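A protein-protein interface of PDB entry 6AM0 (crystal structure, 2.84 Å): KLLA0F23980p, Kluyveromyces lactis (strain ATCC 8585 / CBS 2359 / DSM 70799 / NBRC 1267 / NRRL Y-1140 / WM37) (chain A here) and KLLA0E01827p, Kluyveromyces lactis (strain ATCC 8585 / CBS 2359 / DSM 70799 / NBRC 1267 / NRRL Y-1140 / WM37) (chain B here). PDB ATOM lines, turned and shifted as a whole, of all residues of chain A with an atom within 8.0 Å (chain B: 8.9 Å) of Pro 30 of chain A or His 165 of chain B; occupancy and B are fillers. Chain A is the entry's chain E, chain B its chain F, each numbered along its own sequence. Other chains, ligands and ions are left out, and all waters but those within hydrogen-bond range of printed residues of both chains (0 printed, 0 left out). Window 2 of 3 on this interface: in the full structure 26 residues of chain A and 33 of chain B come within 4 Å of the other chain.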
ATOM      1  N   PHE A  25      20.070  19.134   8.584  1.00  0.00           N
ATOM      2  CA  PHE A  25      21.292  18.566   9.134  1.00  0.00           C
ATOM      3  C   PHE A  25      21.304  17.056   9.311  1.00  0.00           C
ATOM      4  O   PHE A  25      22.395  16.485   9.398  1.00  0.00           O
ATOM      5  CB  PHE A  25      21.607  19.208  10.493  1.00  0.00           C
ATOM      6  CG  PHE A  25      22.002  20.646  10.393  1.00  0.00           C
ATOM      7  CD1 PHE A  25      23.281  20.994   9.997  1.00  0.00           C
ATOM      8  CD2 PHE A  25      21.095  21.652  10.675  1.00  0.00           C
ATOM      9  CE1 PHE A  25      23.651  22.309   9.890  1.00  0.00           C
ATOM     10  CE2 PHE A  25      21.461  22.972  10.572  1.00  0.00           C
ATOM     11  CZ  PHE A  25      22.742  23.300  10.178  1.00  0.00           C
ATOM     12  N   ILE A  26      20.153  16.389   9.395  1.00  0.00           N
ATOM     13  CA  ILE A  26      20.169  14.973   9.753  1.00  0.00           C
ATOM     14  C   ILE A  26      19.336  14.138   8.789  1.00  0.00           C
ATOM     15  O   ILE A  26      19.726  13.022   8.427  1.00  0.00           O
ATOM     16  CB  ILE A  26      19.675  14.758  11.195  1.00  0.00           C
ATOM     17  CG1 ILE A  26      20.230  15.831  12.133  1.00  0.00           C
ATOM     18  CG2 ILE A  26      20.096  13.390  11.692  1.00  0.00           C
ATOM     19  CD1 ILE A  26      19.716  15.733  13.550  1.00  0.00           C
ATOM     20  N   LEU A  27      18.182  14.664   8.373  1.00  0.00           N
ATOM     21  CA  LEU A  27      17.218  13.845   7.645  1.00  0.00           C
ATOM     22  C   LEU A  27      17.753  13.403   6.288  1.00  0.00           C
ATOM     23  O   LEU A  27      17.480  12.282   5.843  1.00  0.00           O
ATOM     24  CB  LEU A  27      15.909  14.610   7.473  1.00  0.00           C
ATOM     25  CG  LEU A  27      14.770  13.844   6.806  1.00  0.00           C
ATOM     26  CD1 LEU A  27      14.536  12.538   7.532  1.00  0.00           C
ATOM     27  CD2 LEU A  27      13.512  14.689   6.800  1.00  0.00           C
ATOM     28  N   ASN A  28      18.520  14.261   5.616  1.00  0.00           N
ATOM     29  CA  ASN A  28      18.874  14.044   4.220  1.00  0.00           C
ATOM     30  C   ASN A  28      20.361  13.803   3.997  1.00  0.00           C
ATOM     31  O   ASN A  28      20.808  13.818   2.847  1.00  0.00           O
ATOM     32  CB  ASN A  28      18.414  15.234   3.379  1.00  0.00           C
ATOM     33  CG  ASN A  28      16.905  15.387   3.361  1.00  0.00           C
ATOM     34  OD1 ASN A  28      16.209  14.697   2.616  1.00  0.00           O
ATOM     35  ND2 ASN A  28      16.393  16.300   4.178  1.00  0.00           N
ATOM     36  N   VAL A  29      21.136  13.580   5.054  1.00  0.00           N
ATOM     37  CA  VAL A  29      22.573  13.350   4.904  1.00  0.00           C
ATOM     38  C   VAL A  29      22.785  12.065   4.114  1.00  0.00           C
ATOM     39  O   VAL A  29      21.924  11.173   4.144  1.00  0.00           O
ATOM     40  CB  VAL A  29      23.284  13.273   6.265  1.00  0.00           C
ATOM     41  CG1 VAL A  29      23.156  14.586   7.009  1.00  0.00           C
ATOM     42  CG2 VAL A  29      22.732  12.123   7.090  1.00  0.00           C
ATOM     43  N   PRO A  30      23.890  11.930   3.388  1.00  0.00           N
ATOM     44  CA  PRO A  30      24.184  10.664   2.708  1.00  0.00           C
ATOM     45  C   PRO A  30      24.307   9.534   3.713  1.00  0.00           C
ATOM     46  O   PRO A  30      24.596   9.779   4.895  1.00  0.00           O
ATOM     47  CB  PRO A  30      25.521  10.941   2.000  1.00  0.00           C
ATOM     48  CG  PRO A  30      26.071  12.169   2.652  1.00  0.00           C
ATOM     49  CD  PRO A  30      24.892  12.967   3.089  1.00  0.00           C
ATOM     50  N   PRO A  31      24.077   8.285   3.293  1.00  0.00           N
ATOM     51  CA  PRO A  31      24.058   7.182   4.269  1.00  0.00           C
ATOM     52  C   PRO A  31      25.374   6.998   4.999  1.00  0.00           C
ATOM     53  O   PRO A  31      25.377   6.518   6.139  1.00  0.00           O
ATOM     54  CB  PRO A  31      23.712   5.957   3.407  1.00  0.00           C
ATOM     55  CG  PRO A  31      24.110   6.338   2.024  1.00  0.00           C
ATOM     56  CD  PRO A  31      23.844   7.810   1.918  1.00  0.00           C
ATOM     57  N   GLU A  32      26.489   7.380   4.373  1.00  0.00           N
ATOM     58  CA  GLU A  32      27.797   7.293   5.016  1.00  0.00           C
ATOM     59  C   GLU A  32      27.819   8.006   6.366  1.00  0.00           C
ATOM     60  O   GLU A  32      28.556   7.599   7.272  1.00  0.00           O
ATOM     61  CB  GLU A  32      28.853   7.863   4.062  1.00  0.00           C
ATOM     62  CG  GLU A  32      30.144   8.361   4.695  1.00  0.00           C
ATOM     63  CD  GLU A  32      31.135   7.253   5.001  1.00  0.00           C
ATOM     64  OE1 GLU A  32      30.752   6.272   5.672  1.00  0.00           O
ATOM     65  OE2 GLU A  32      32.303   7.366   4.567  1.00  0.00           O
ATOM     66  N   ASP A  33      27.000   9.043   6.533  1.00  0.00           N
ATOM     67  CA  ASP A  33      26.965   9.831   7.757  1.00  0.00           C
ATOM     68  C   ASP A  33      25.987   9.296   8.797  1.00  0.00           C
ATOM     69  O   ASP A  33      25.912   9.851   9.898  1.00  0.00           O
ATOM     70  CB  ASP A  33      26.615  11.281   7.428  1.00  0.00           C
ATOM     71  CG  ASP A  33      27.667  11.947   6.573  1.00  0.00           C
ATOM     72  OD1 ASP A  33      27.733  11.634   5.366  1.00  0.00           O
ATOM     73  OD2 ASP A  33      28.428  12.783   7.105  1.00  0.00           O
ATOM     74  N   LEU A  34      25.232   8.245   8.476  1.00  0.00           N
ATOM     75  CA  LEU A  34      24.313   7.618   9.418  1.00  0.00           C
ATOM     76  C   LEU A  34      24.802   6.242   9.861  1.00  0.00           C
ATOM     77  O   LEU A  34      24.022   5.455  10.403  1.00  0.00           O
ATOM     78  CB  LEU A  34      22.915   7.514   8.804  1.00  0.00           C
ATOM     79  CG  LEU A  34      22.172   8.816   8.495  1.00  0.00           C
ATOM     80  CD1 LEU A  34      21.130   8.596   7.410  1.00  0.00           C
ATOM     81  CD2 LEU A  34      21.520   9.377   9.746  1.00  0.00           C
ATOM     82  N   SER A  35      26.089   5.949   9.652  1.00  0.00           N
ATOM     83  CA  SER A  35      26.594   4.594   9.858  1.00  0.00           C
ATOM     84  C   SER A  35      26.637   4.227  11.337  1.00  0.00           C
ATOM     85  O   SER A  35      26.167   3.154  11.732  1.00  0.00           O
ATOM     86  CB  SER A  35      27.980   4.457   9.223  1.00  0.00           C
ATOM     87  OG  SER A  35      28.780   5.598   9.482  1.00  0.00           O
ATOM     88  N   HIS A  43      26.383  15.466  13.283  1.00  0.00           N
ATOM     89  CA  HIS A  43      25.325  16.243  12.647  1.00  0.00           C
ATOM     90  C   HIS A  43      24.374  16.825  13.685  1.00  0.00           C
ATOM     91  O   HIS A  43      23.909  17.963  13.541  1.00  0.00           O
ATOM     92  CB  HIS A  43      24.576  15.376  11.642  1.00  0.00           C
ATOM     93  CG  HIS A  43      25.394  15.014  10.445  1.00  0.00           C
ATOM     94  ND1 HIS A  43      25.652  15.907   9.428  1.00  0.00           N
ATOM     95  CD2 HIS A  43      26.022  13.865  10.105  1.00  0.00           C
ATOM     96  CE1 HIS A  43      26.399  15.322   8.509  1.00  0.00           C
ATOM     97  NE2 HIS A  43      26.639  14.082   8.897  1.00  0.00           N
ATOM     98  N   ARG B  12      10.746  11.145   5.038  1.00  0.00           N
ATOM     99  CA  ARG B  12      11.702  12.088   4.473  1.00  0.00           C
ATOM    100  C   ARG B  12      11.035  12.977   3.433  1.00  0.00           C
ATOM    101  O   ARG B  12      11.144  14.208   3.491  1.00  0.00           O
ATOM    102  CB  ARG B  12      12.889  11.332   3.876  1.00  0.00           C
ATOM    103  CG  ARG B  12      13.925  12.219   3.207  1.00  0.00           C
ATOM    104  CD  ARG B  12      15.342  11.694   3.418  1.00  0.00           C
ATOM    105  NE  ARG B  12      15.491  10.291   3.039  1.00  0.00           N
ATOM    106  CZ  ARG B  12      15.655   9.294   3.904  1.00  0.00           C
ATOM    107  NH1 ARG B  12      15.697   9.539   5.207  1.00  0.00           N
ATOM    108  NH2 ARG B  12      15.778   8.049   3.465  1.00  0.00           N
ATOM    109  N   HIS B  33      15.357  14.878  -5.429  1.00  0.00           N
ATOM    110  CA  HIS B  33      16.097  15.188  -4.216  1.00  0.00           C
ATOM    111  C   HIS B  33      17.440  14.470  -4.258  1.00  0.00           C
ATOM    112  O   HIS B  33      17.516  13.310  -4.673  1.00  0.00           O
ATOM    113  CB  HIS B  33      15.289  14.785  -2.975  1.00  0.00           C
ATOM    114  CG  HIS B  33      16.063  13.980  -1.981  1.00  0.00           C
ATOM    115  ND1 HIS B  33      16.382  12.653  -2.181  1.00  0.00           N
ATOM    116  CD2 HIS B  33      16.570  14.311  -0.770  1.00  0.00           C
ATOM    117  CE1 HIS B  33      17.064  12.206  -1.142  1.00  0.00           C
ATOM    118  NE2 HIS B  33      17.189  13.191  -0.271  1.00  0.00           N
ATOM    119  N   THR B  34      18.496  15.170  -3.839  1.00  0.00           N
ATOM    120  CA  THR B  34      19.829  14.599  -3.718  1.00  0.00           C
ATOM    121  C   THR B  34      20.432  14.980  -2.373  1.00  0.00           C
ATOM    122  O   THR B  34      20.245  16.112  -1.894  1.00  0.00           O
ATOM    123  CB  THR B  34      20.754  15.056  -4.864  1.00  0.00           C
ATOM    124  OG1 THR B  34      22.023  14.401  -4.744  1.00  0.00           O
ATOM    125  CG2 THR B  34      20.974  16.548  -4.830  1.00  0.00           C
ATOM    126  N   PRO B  35      21.163  14.050  -1.744  1.00  0.00           N
ATOM    127  CA  PRO B  35      21.583  14.255  -0.345  1.00  0.00           C
ATOM    128  C   PRO B  35      22.422  15.497  -0.109  1.00  0.00           C
ATOM    129  O   PRO B  35      22.212  16.188   0.894  1.00  0.00           O
ATOM    130  CB  PRO B  35      22.379  12.979  -0.036  1.00  0.00           C
ATOM    131  CG  PRO B  35      21.857  11.966  -0.987  1.00  0.00           C
ATOM    132  CD  PRO B  35      21.525  12.710  -2.239  1.00  0.00           C
ATOM    133  N   HIS B  36      23.377  15.801  -0.980  1.00  0.00           N
ATOM    134  CA  HIS B  36      24.260  16.927  -0.720  1.00  0.00           C
ATOM    135  C   HIS B  36      24.619  17.622  -2.022  1.00  0.00           C
ATOM    136  O   HIS B  36      24.775  16.973  -3.060  1.00  0.00           O
ATOM    137  CB  HIS B  36      25.530  16.478   0.009  1.00  0.00           C
ATOM    138  CG  HIS B  36      26.271  17.598   0.665  1.00  0.00           C
ATOM    139  ND1 HIS B  36      27.534  17.984   0.273  1.00  0.00           N
ATOM    140  CD2 HIS B  36      25.922  18.424   1.680  1.00  0.00           C
ATOM    141  CE1 HIS B  36      27.933  18.997   1.021  1.00  0.00           C
ATOM    142  NE2 HIS B  36      26.974  19.282   1.884  1.00  0.00           N
ATOM    143  N   ALA B  37      24.740  18.946  -1.959  1.00  0.00           N
ATOM    144  CA  ALA B  37      25.121  19.739  -3.118  1.00  0.00           C
ATOM    145  C   ALA B  37      25.840  20.996  -2.651  1.00  0.00           C
ATOM    146  O   ALA B  37      25.462  21.596  -1.641  1.00  0.00           O
ATOM    147  CB  ALA B  37      23.904  20.115  -3.969  1.00  0.00           C
ATOM    148  N   THR B  38      26.876  21.382  -3.391  1.00  0.00           N
ATOM    149  CA  THR B  38      27.653  22.584  -3.115  1.00  0.00           C
ATOM    150  C   THR B  38      27.526  23.543  -4.294  1.00  0.00           C
ATOM    151  O   THR B  38      27.457  23.111  -5.449  1.00  0.00           O
ATOM    152  CB  THR B  38      29.131  22.240  -2.859  1.00  0.00           C
ATOM    153  OG1 THR B  38      29.217  21.145  -1.939  1.00  0.00           O
ATOM    154  CG2 THR B  38      29.872  23.436  -2.275  1.00  0.00           C
ATOM    155  N   GLN B  53      25.225  24.991   1.138  1.00  0.00           N
ATOM    156  CA  GLN B  53      25.592  23.583   1.221  1.00  0.00           C
ATOM    157  C   GLN B  53      24.514  22.778   1.938  1.00  0.00           C
ATOM    158  O   GLN B  53      24.122  23.122   3.059  1.00  0.00           O
ATOM    159  CB  GLN B  53      26.923  23.430   1.952  1.00  0.00           C
ATOM    160  CG  GLN B  53      27.811  22.352   1.387  1.00  0.00           C
ATOM    161  CD  GLN B  53      29.064  22.163   2.204  1.00  0.00           C
ATOM    162  OE1 GLN B  53      29.168  22.670   3.321  1.00  0.00           O
ATOM    163  NE2 GLN B  53      30.028  21.433   1.653  1.00  0.00           N
ATOM    164  N   GLY B  54      24.040  21.707   1.318  1.00  0.00           N
ATOM    165  CA  GLY B  54      23.030  20.877   1.939  1.00  0.00           C
ATOM    166  C   GLY B  54      22.260  20.079   0.905  1.00  0.00           C
ATOM    167  O   GLY B  54      22.651  19.984  -0.260  1.00  0.00           O
ATOM    168  N   VAL B  55      21.154  19.496   1.373  1.00  0.00           N
ATOM    169  CA  VAL B  55      20.311  18.685   0.506  1.00  0.00           C
ATOM    170  C   VAL B  55      19.695  19.559  -0.573  1.00  0.00           C
ATOM    171  O   VAL B  55      19.282  20.698  -0.320  1.00  0.00           O
ATOM    172  CB  VAL B  55      19.231  17.973   1.336  1.00  0.00           C
ATOM    173  CG1 VAL B  55      18.537  18.963   2.259  1.00  0.00           C
ATOM    174  CG2 VAL B  55      18.225  17.285   0.432  1.00  0.00           C
ATOM    175  N   LEU B  56      19.644  19.035  -1.792  1.00  0.00           N
ATOM    176  CA  LEU B  56      19.087  19.770  -2.918  1.00  0.00           C
ATOM    177  C   LEU B  56      17.799  19.105  -3.373  1.00  0.00           C
ATOM    178  O   LEU B  56      17.693  17.876  -3.379  1.00  0.00           O
ATOM    179  CB  LEU B  56      20.089  19.844  -4.074  1.00  0.00           C
ATOM    180  CG  LEU B  56      19.672  20.498  -5.391  1.00  0.00           C
ATOM    181  CD1 LEU B  56      20.884  21.159  -6.007  1.00  0.00           C
ATOM    182  CD2 LEU B  56      19.085  19.484  -6.362  1.00  0.00           C
ATOM    183  N   ARG B 108      23.122  24.260   5.191  1.00  0.00           N
ATOM    184  CA  ARG B 108      23.700  23.896   6.477  1.00  0.00           C
ATOM    185  C   ARG B 108      24.601  24.982   7.044  1.00  0.00           C
ATOM    186  O   ARG B 108      24.852  24.995   8.254  1.00  0.00           O
ATOM    187  CB  ARG B 108      24.519  22.607   6.350  1.00  0.00           C
ATOM    188  CG  ARG B 108      23.765  21.406   5.825  1.00  0.00           C
ATOM    189  CD  ARG B 108      24.700  20.219   5.689  1.00  0.00           C
ATOM    190  NE  ARG B 108      25.362  19.913   6.954  1.00  0.00           N
ATOM    191  CZ  ARG B 108      25.108  18.837   7.693  1.00  0.00           C
ATOM    192  NH1 ARG B 108      24.207  17.949   7.292  1.00  0.00           N
ATOM    193  NH2 ARG B 108      25.760  18.645   8.831  1.00  0.00           N
ATOM    194  N   ASP B 148      31.826  16.487 -14.299  1.00  0.00           N
ATOM    195  CA  ASP B 148      31.007  16.202 -13.126  1.00  0.00           C
ATOM    196  C   ASP B 148      30.456  17.457 -12.456  1.00  0.00           C
ATOM    197  O   ASP B 148      29.995  17.395 -11.313  1.00  0.00           O
ATOM    198  CB  ASP B 148      31.777  15.350 -12.106  1.00  0.00           C
ATOM    199  CG  ASP B 148      32.347  14.079 -12.720  1.00  0.00           C
ATOM    200  OD1 ASP B 148      31.563  13.142 -12.994  1.00  0.00           O
ATOM    201  OD2 ASP B 148      33.578  14.016 -12.928  1.00  0.00           O
ATOM    202  N   ILE B 162      26.587  23.748  -9.760  1.00  0.00           N
ATOM    203  CA  ILE B 162      26.188  22.874  -8.671  1.00  0.00           C
ATOM    204  C   ILE B 162      27.004  21.597  -8.765  1.00  0.00           C
ATOM    205  O   ILE B 162      27.129  21.002  -9.846  1.00  0.00           O
ATOM    206  CB  ILE B 162      24.678  22.584  -8.717  1.00  0.00           C
ATOM    207  CG1 ILE B 162      23.895  23.838  -8.315  1.00  0.00           C
ATOM    208  CG2 ILE B 162      24.325  21.402  -7.825  1.00  0.00           C
ATOM    209  CD1 ILE B 162      22.749  24.174  -9.240  1.00  0.00           C
ATOM    210  N   TRP B 163      27.585  21.198  -7.641  1.00  0.00           N
ATOM    211  CA  TRP B 163      28.378  19.982  -7.540  1.00  0.00           C
ATOM    212  C   TRP B 163      27.657  19.044  -6.584  1.00  0.00           C
ATOM    213  O   TRP B 163      27.529  19.337  -5.390  1.00  0.00           O
ATOM    214  CB  TRP B 163      29.793  20.291  -7.062  1.00  0.00           C
ATOM    215  CG  TRP B 163      30.716  19.122  -7.143  1.00  0.00           C
ATOM    216  CD1 TRP B 163      31.541  18.798  -8.183  1.00  0.00           C
ATOM    217  CD2 TRP B 163      30.915  18.119  -6.144  1.00  0.00           C
ATOM    218  NE1 TRP B 163      32.240  17.654  -7.890  1.00  0.00           N
ATOM    219  CE2 TRP B 163      31.874  17.217  -6.644  1.00  0.00           C
ATOM    220  CE3 TRP B 163      30.373  17.894  -4.874  1.00  0.00           C
ATOM    221  CZ2 TRP B 163      32.305  16.109  -5.919  1.00  0.00           C
ATOM    222  CZ3 TRP B 163      30.802  16.794  -4.156  1.00  0.00           C
ATOM    223  CH2 TRP B 163      31.758  15.914  -4.680  1.00  0.00           C
ATOM    224  N   VAL B 164      27.187  17.934  -7.110  1.00  0.00           N
ATOM    225  CA  VAL B 164      26.401  16.980  -6.344  1.00  0.00           C
ATOM    226  C   VAL B 164      27.330  15.934  -5.750  1.00  0.00           C
ATOM    227  O   VAL B 164      28.253  15.448  -6.415  1.00  0.00           O
ATOM    228  CB  VAL B 164      25.316  16.341  -7.231  1.00  0.00           C
ATOM    229  CG1 VAL B 164      24.632  15.204  -6.503  1.00  0.00           C
ATOM    230  CG2 VAL B 164      24.301  17.393  -7.643  1.00  0.00           C
ATOM    231  N   HIS B 165      27.092  15.596  -4.482  1.00  0.00           N
ATOM    232  CA  HIS B 165      27.890  14.579  -3.809  1.00  0.00           C
ATOM    233  C   HIS B 165      27.783  13.234  -4.521  1.00  0.00           C
ATOM    234  O   HIS B 165      28.786  12.682  -4.988  1.00  0.00           O
ATOM    235  CB  HIS B 165      27.448  14.454  -2.353  1.00  0.00           C
ATOM    236  CG  HIS B 165      27.956  13.223  -1.673  1.00  0.00           C
ATOM    237  ND1 HIS B 165      29.271  13.073  -1.291  1.00  0.00           N
ATOM    238  CD2 HIS B 165      27.329  12.077  -1.317  1.00  0.00           C
ATOM    239  CE1 HIS B 165      29.431  11.892  -0.721  1.00  0.00           C
ATOM    240  NE2 HIS B 165      28.267  11.267  -0.726  1.00  0.00           N
ATOM    241  N   THR B 166      26.577  12.689  -4.607  1.00  0.00           N
ATOM    242  CA  THR B 166      26.389  11.374  -5.216  1.00  0.00           C
ATOM    243  C   THR B 166      26.574  11.477  -6.725  1.00  0.00           C
ATOM    244  O   THR B 166      25.840  12.231  -7.380  1.00  0.00           O
ATOM    245  CB  THR B 166      25.008  10.815  -4.873  1.00  0.00           C
ATOM    246  OG1 THR B 166      23.998  11.570  -5.551  1.00  0.00           O
ATOM    247  CG2 THR B 166      24.761  10.895  -3.371  1.00  0.00           C
ATOM    248  N   PRO B 167      27.530  10.752  -7.318  1.00  0.00           N
ATOM    249  CA  PRO B 167      27.864  11.010  -8.731  1.00  0.00           C
ATOM    250  C   PRO B 167      26.755  10.665  -9.711  1.00  0.00           C
ATOM    251  O   PRO B 167      26.511  11.437 -10.648  1.00  0.00           O
ATOM    252  CB  PRO B 167      29.115  10.146  -8.956  1.00  0.00           C
ATOM    253  CG  PRO B 167      29.073   9.114  -7.879  1.00  0.00           C
ATOM    254  CD  PRO B 167      28.449   9.785  -6.696  1.00  0.00           C
ATOM    255  N   GLU B 168      26.073   9.531  -9.536  1.00  0.00           N
ATOM    256  CA  GLU B 168      25.053   9.139 -10.504  1.00  0.00           C
ATOM    257  C   GLU B 168      23.856  10.083 -10.518  1.00  0.00           C
ATOM    258  O   GLU B 168      23.025   9.982 -11.427  1.00  0.00           O
ATOM    259  CB  GLU B 168      24.579   7.705 -10.244  1.00  0.00           C
ATOM    260  CG  GLU B 168      23.998   7.456  -8.861  1.00  0.00           C
ATOM    261  CD  GLU B 168      25.062   7.161  -7.820  1.00  0.00           C
ATOM    262  OE1 GLU B 168      26.254   7.082  -8.190  1.00  0.00           O
ATOM    263  OE2 GLU B 168      24.707   7.006  -6.633  1.00  0.00           O
ATOM    264  N   ASP B 169      23.749  10.994  -9.547  1.00  0.00           N
ATOM    265  CA  ASP B 169      22.707  12.013  -9.581  1.00  0.00           C
ATOM    266  C   ASP B 169      23.089  13.217 -10.431  1.00  0.00           C
ATOM    267  O   ASP B 169      22.195  13.938 -10.892  1.00  0.00           O
ATOM    268  CB  ASP B 169      22.370  12.491  -8.166  1.00  0.00           C
ATOM    269  CG  ASP B 169      21.495  11.509  -7.407  1.00  0.00           C
ATOM    270  OD1 ASP B 169      20.958  10.574  -8.039  1.00  0.00           O
ATOM    271  OD2 ASP B 169      21.335  11.685  -6.179  1.00  0.00           O
ATOM    272  N   ARG B 170      24.386  13.450 -10.647  1.00  0.00           N
ATOM    273  CA  ARG B 170      24.824  14.621 -11.402  1.00  0.00           C
ATOM    274  C   ARG B 170      24.151  14.666 -12.768  1.00  0.00           C
ATOM    275  O   ARG B 170      23.392  15.595 -13.074  1.00  0.00           O
ATOM    276  CB  ARG B 170      26.347  14.610 -11.529  1.00  0.00           C
ATOM    277  CG  ARG B 170      27.044  14.463 -10.188  1.00  0.00           C
ATOM    278  CD  ARG B 170      28.531  14.742 -10.267  1.00  0.00           C
ATOM    279  NE  ARG B 170      29.127  14.735  -8.934  1.00  0.00           N
ATOM    280  CZ  ARG B 170      29.985  13.817  -8.502  1.00  0.00           C
ATOM    281  NH1 ARG B 170      30.370  12.836  -9.307  1.00  0.00           N
ATOM    282  NH2 ARG B 170      30.467  13.888  -7.270  1.00  0.00           N
ATOM    283  N   ILE B 173      20.512  15.168 -12.500  1.00  0.00           N
ATOM    284  CA  ILE B 173      20.091  16.560 -12.356  1.00  0.00           C
ATOM    285  C   ILE B 173      19.940  17.195 -13.728  1.00  0.00           C
ATOM    286  O   ILE B 173      18.879  17.729 -14.081  1.00  0.00           O
ATOM    287  CB  ILE B 173      21.090  17.344 -11.487  1.00  0.00           C
ATOM    288  CG1 ILE B 173      20.902  16.996 -10.015  1.00  0.00           C
ATOM    289  CG2 ILE B 173      20.903  18.840 -11.694  1.00  0.00           C
ATOM    290  CD1 ILE B 173      19.686  17.648  -9.411  1.00  0.00           C
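ND1 of His 43 of chain A sits at hydrogen-bond distance from NH2 of Arg 108 of chain B, 2.8 Å away.
The backbone carbonyl oxygen (O) of Phe 25 of chain A is in hydrogen-bond range of the guanidinium group (NH1) of Arg 108 of chain B (3.1 Å).
The backbone carbonyl oxygen (O) of Pro 35 of chain B lies close to the backbone carbonyl oxygen (O) of Asn 28 of chain A.
NE2 of His 33 of chain B lies within hydrogen-bond range of OD1 of Asn 28 of chain A, 3.4 Å away.
The backbone carbonyl oxygen (O) of Leu 27 of chain A sits close to the guanidinium group (NH1) of Arg 12 of chain B (3.3 Å).
OD2 of Asp 33 of chain A lies within hydrogen-bond range of NE2 of His 43 of chain A, 2.8 Å away.
N of His 165 of chain B sits at hydrogen-bond distance from O of His 36 of chain B.
The backbone carbonyl oxygen (O) of Gln 53 of chain B lies within hydrogen-bond range of the backbone NH (N) of Arg 108 of chain B (2.6 Å).
The guanidinium group (NH2) of Arg 170 of chain B sits at hydrogen-bond distance from the backbone carbonyl oxygen (O) of His 165 of chain B (3.1 Å).
The backbone carbonyl oxygen (O) of Phe 25 of chain A is in hydrogen-bond range of a ring nitrogen (ND1) of His 43 of chain A.
Asn 28 of chain A touches Arg 12 of chain B (OD1 to CD, 3.2 Å).
CB of Val 55 of chain B touches CB of Asn 28 of chain A, at 3.5 Å.
Arg 108 of chain B touches Val 29 of chain A.
Pro 35 of chain B touches Pro 30 of chain A (CB to N, 3.9 Å).
Pro 30 of chain A touches His 165 of chain B (CB to NE2, 3.9 Å).
Ile 26 of chain A touches none of the printed residues of chain B.
Printed residues of chain B within 4 Å of Leu 27 of chain A: Arg 12 (3.3 Å).
Val 29 of chain A touches one residue of chain B.
Of chain B, only Pro 35 and His 165 come within 4 Å of Pro 30 of chain A.
No residue of chain B comes within 4 Å of Pro 31 of chain A.
Printed residues of chain B within 4 Å of His 43 of chain A: Arg 108 (2.8 Å).
Of the printed residues of chain A, Arg 12 of chain B touches Leu 27 and Asn 28.
Of chain A, only Pro 30 comes within 4 Å of His 165 of chain B.
Hydrophobic or aromatic side chains of chain A that line the printed part of chain B: Phe 25, Leu 27, Val 29, Pro 30 and His 43.
Among the printed residues, 10 pairs touch across the chains.
Among the printed residues, no Asp or Glu carboxylate lies within 4 Å of a Lys or Arg side-chain nitrogen of the other chain.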
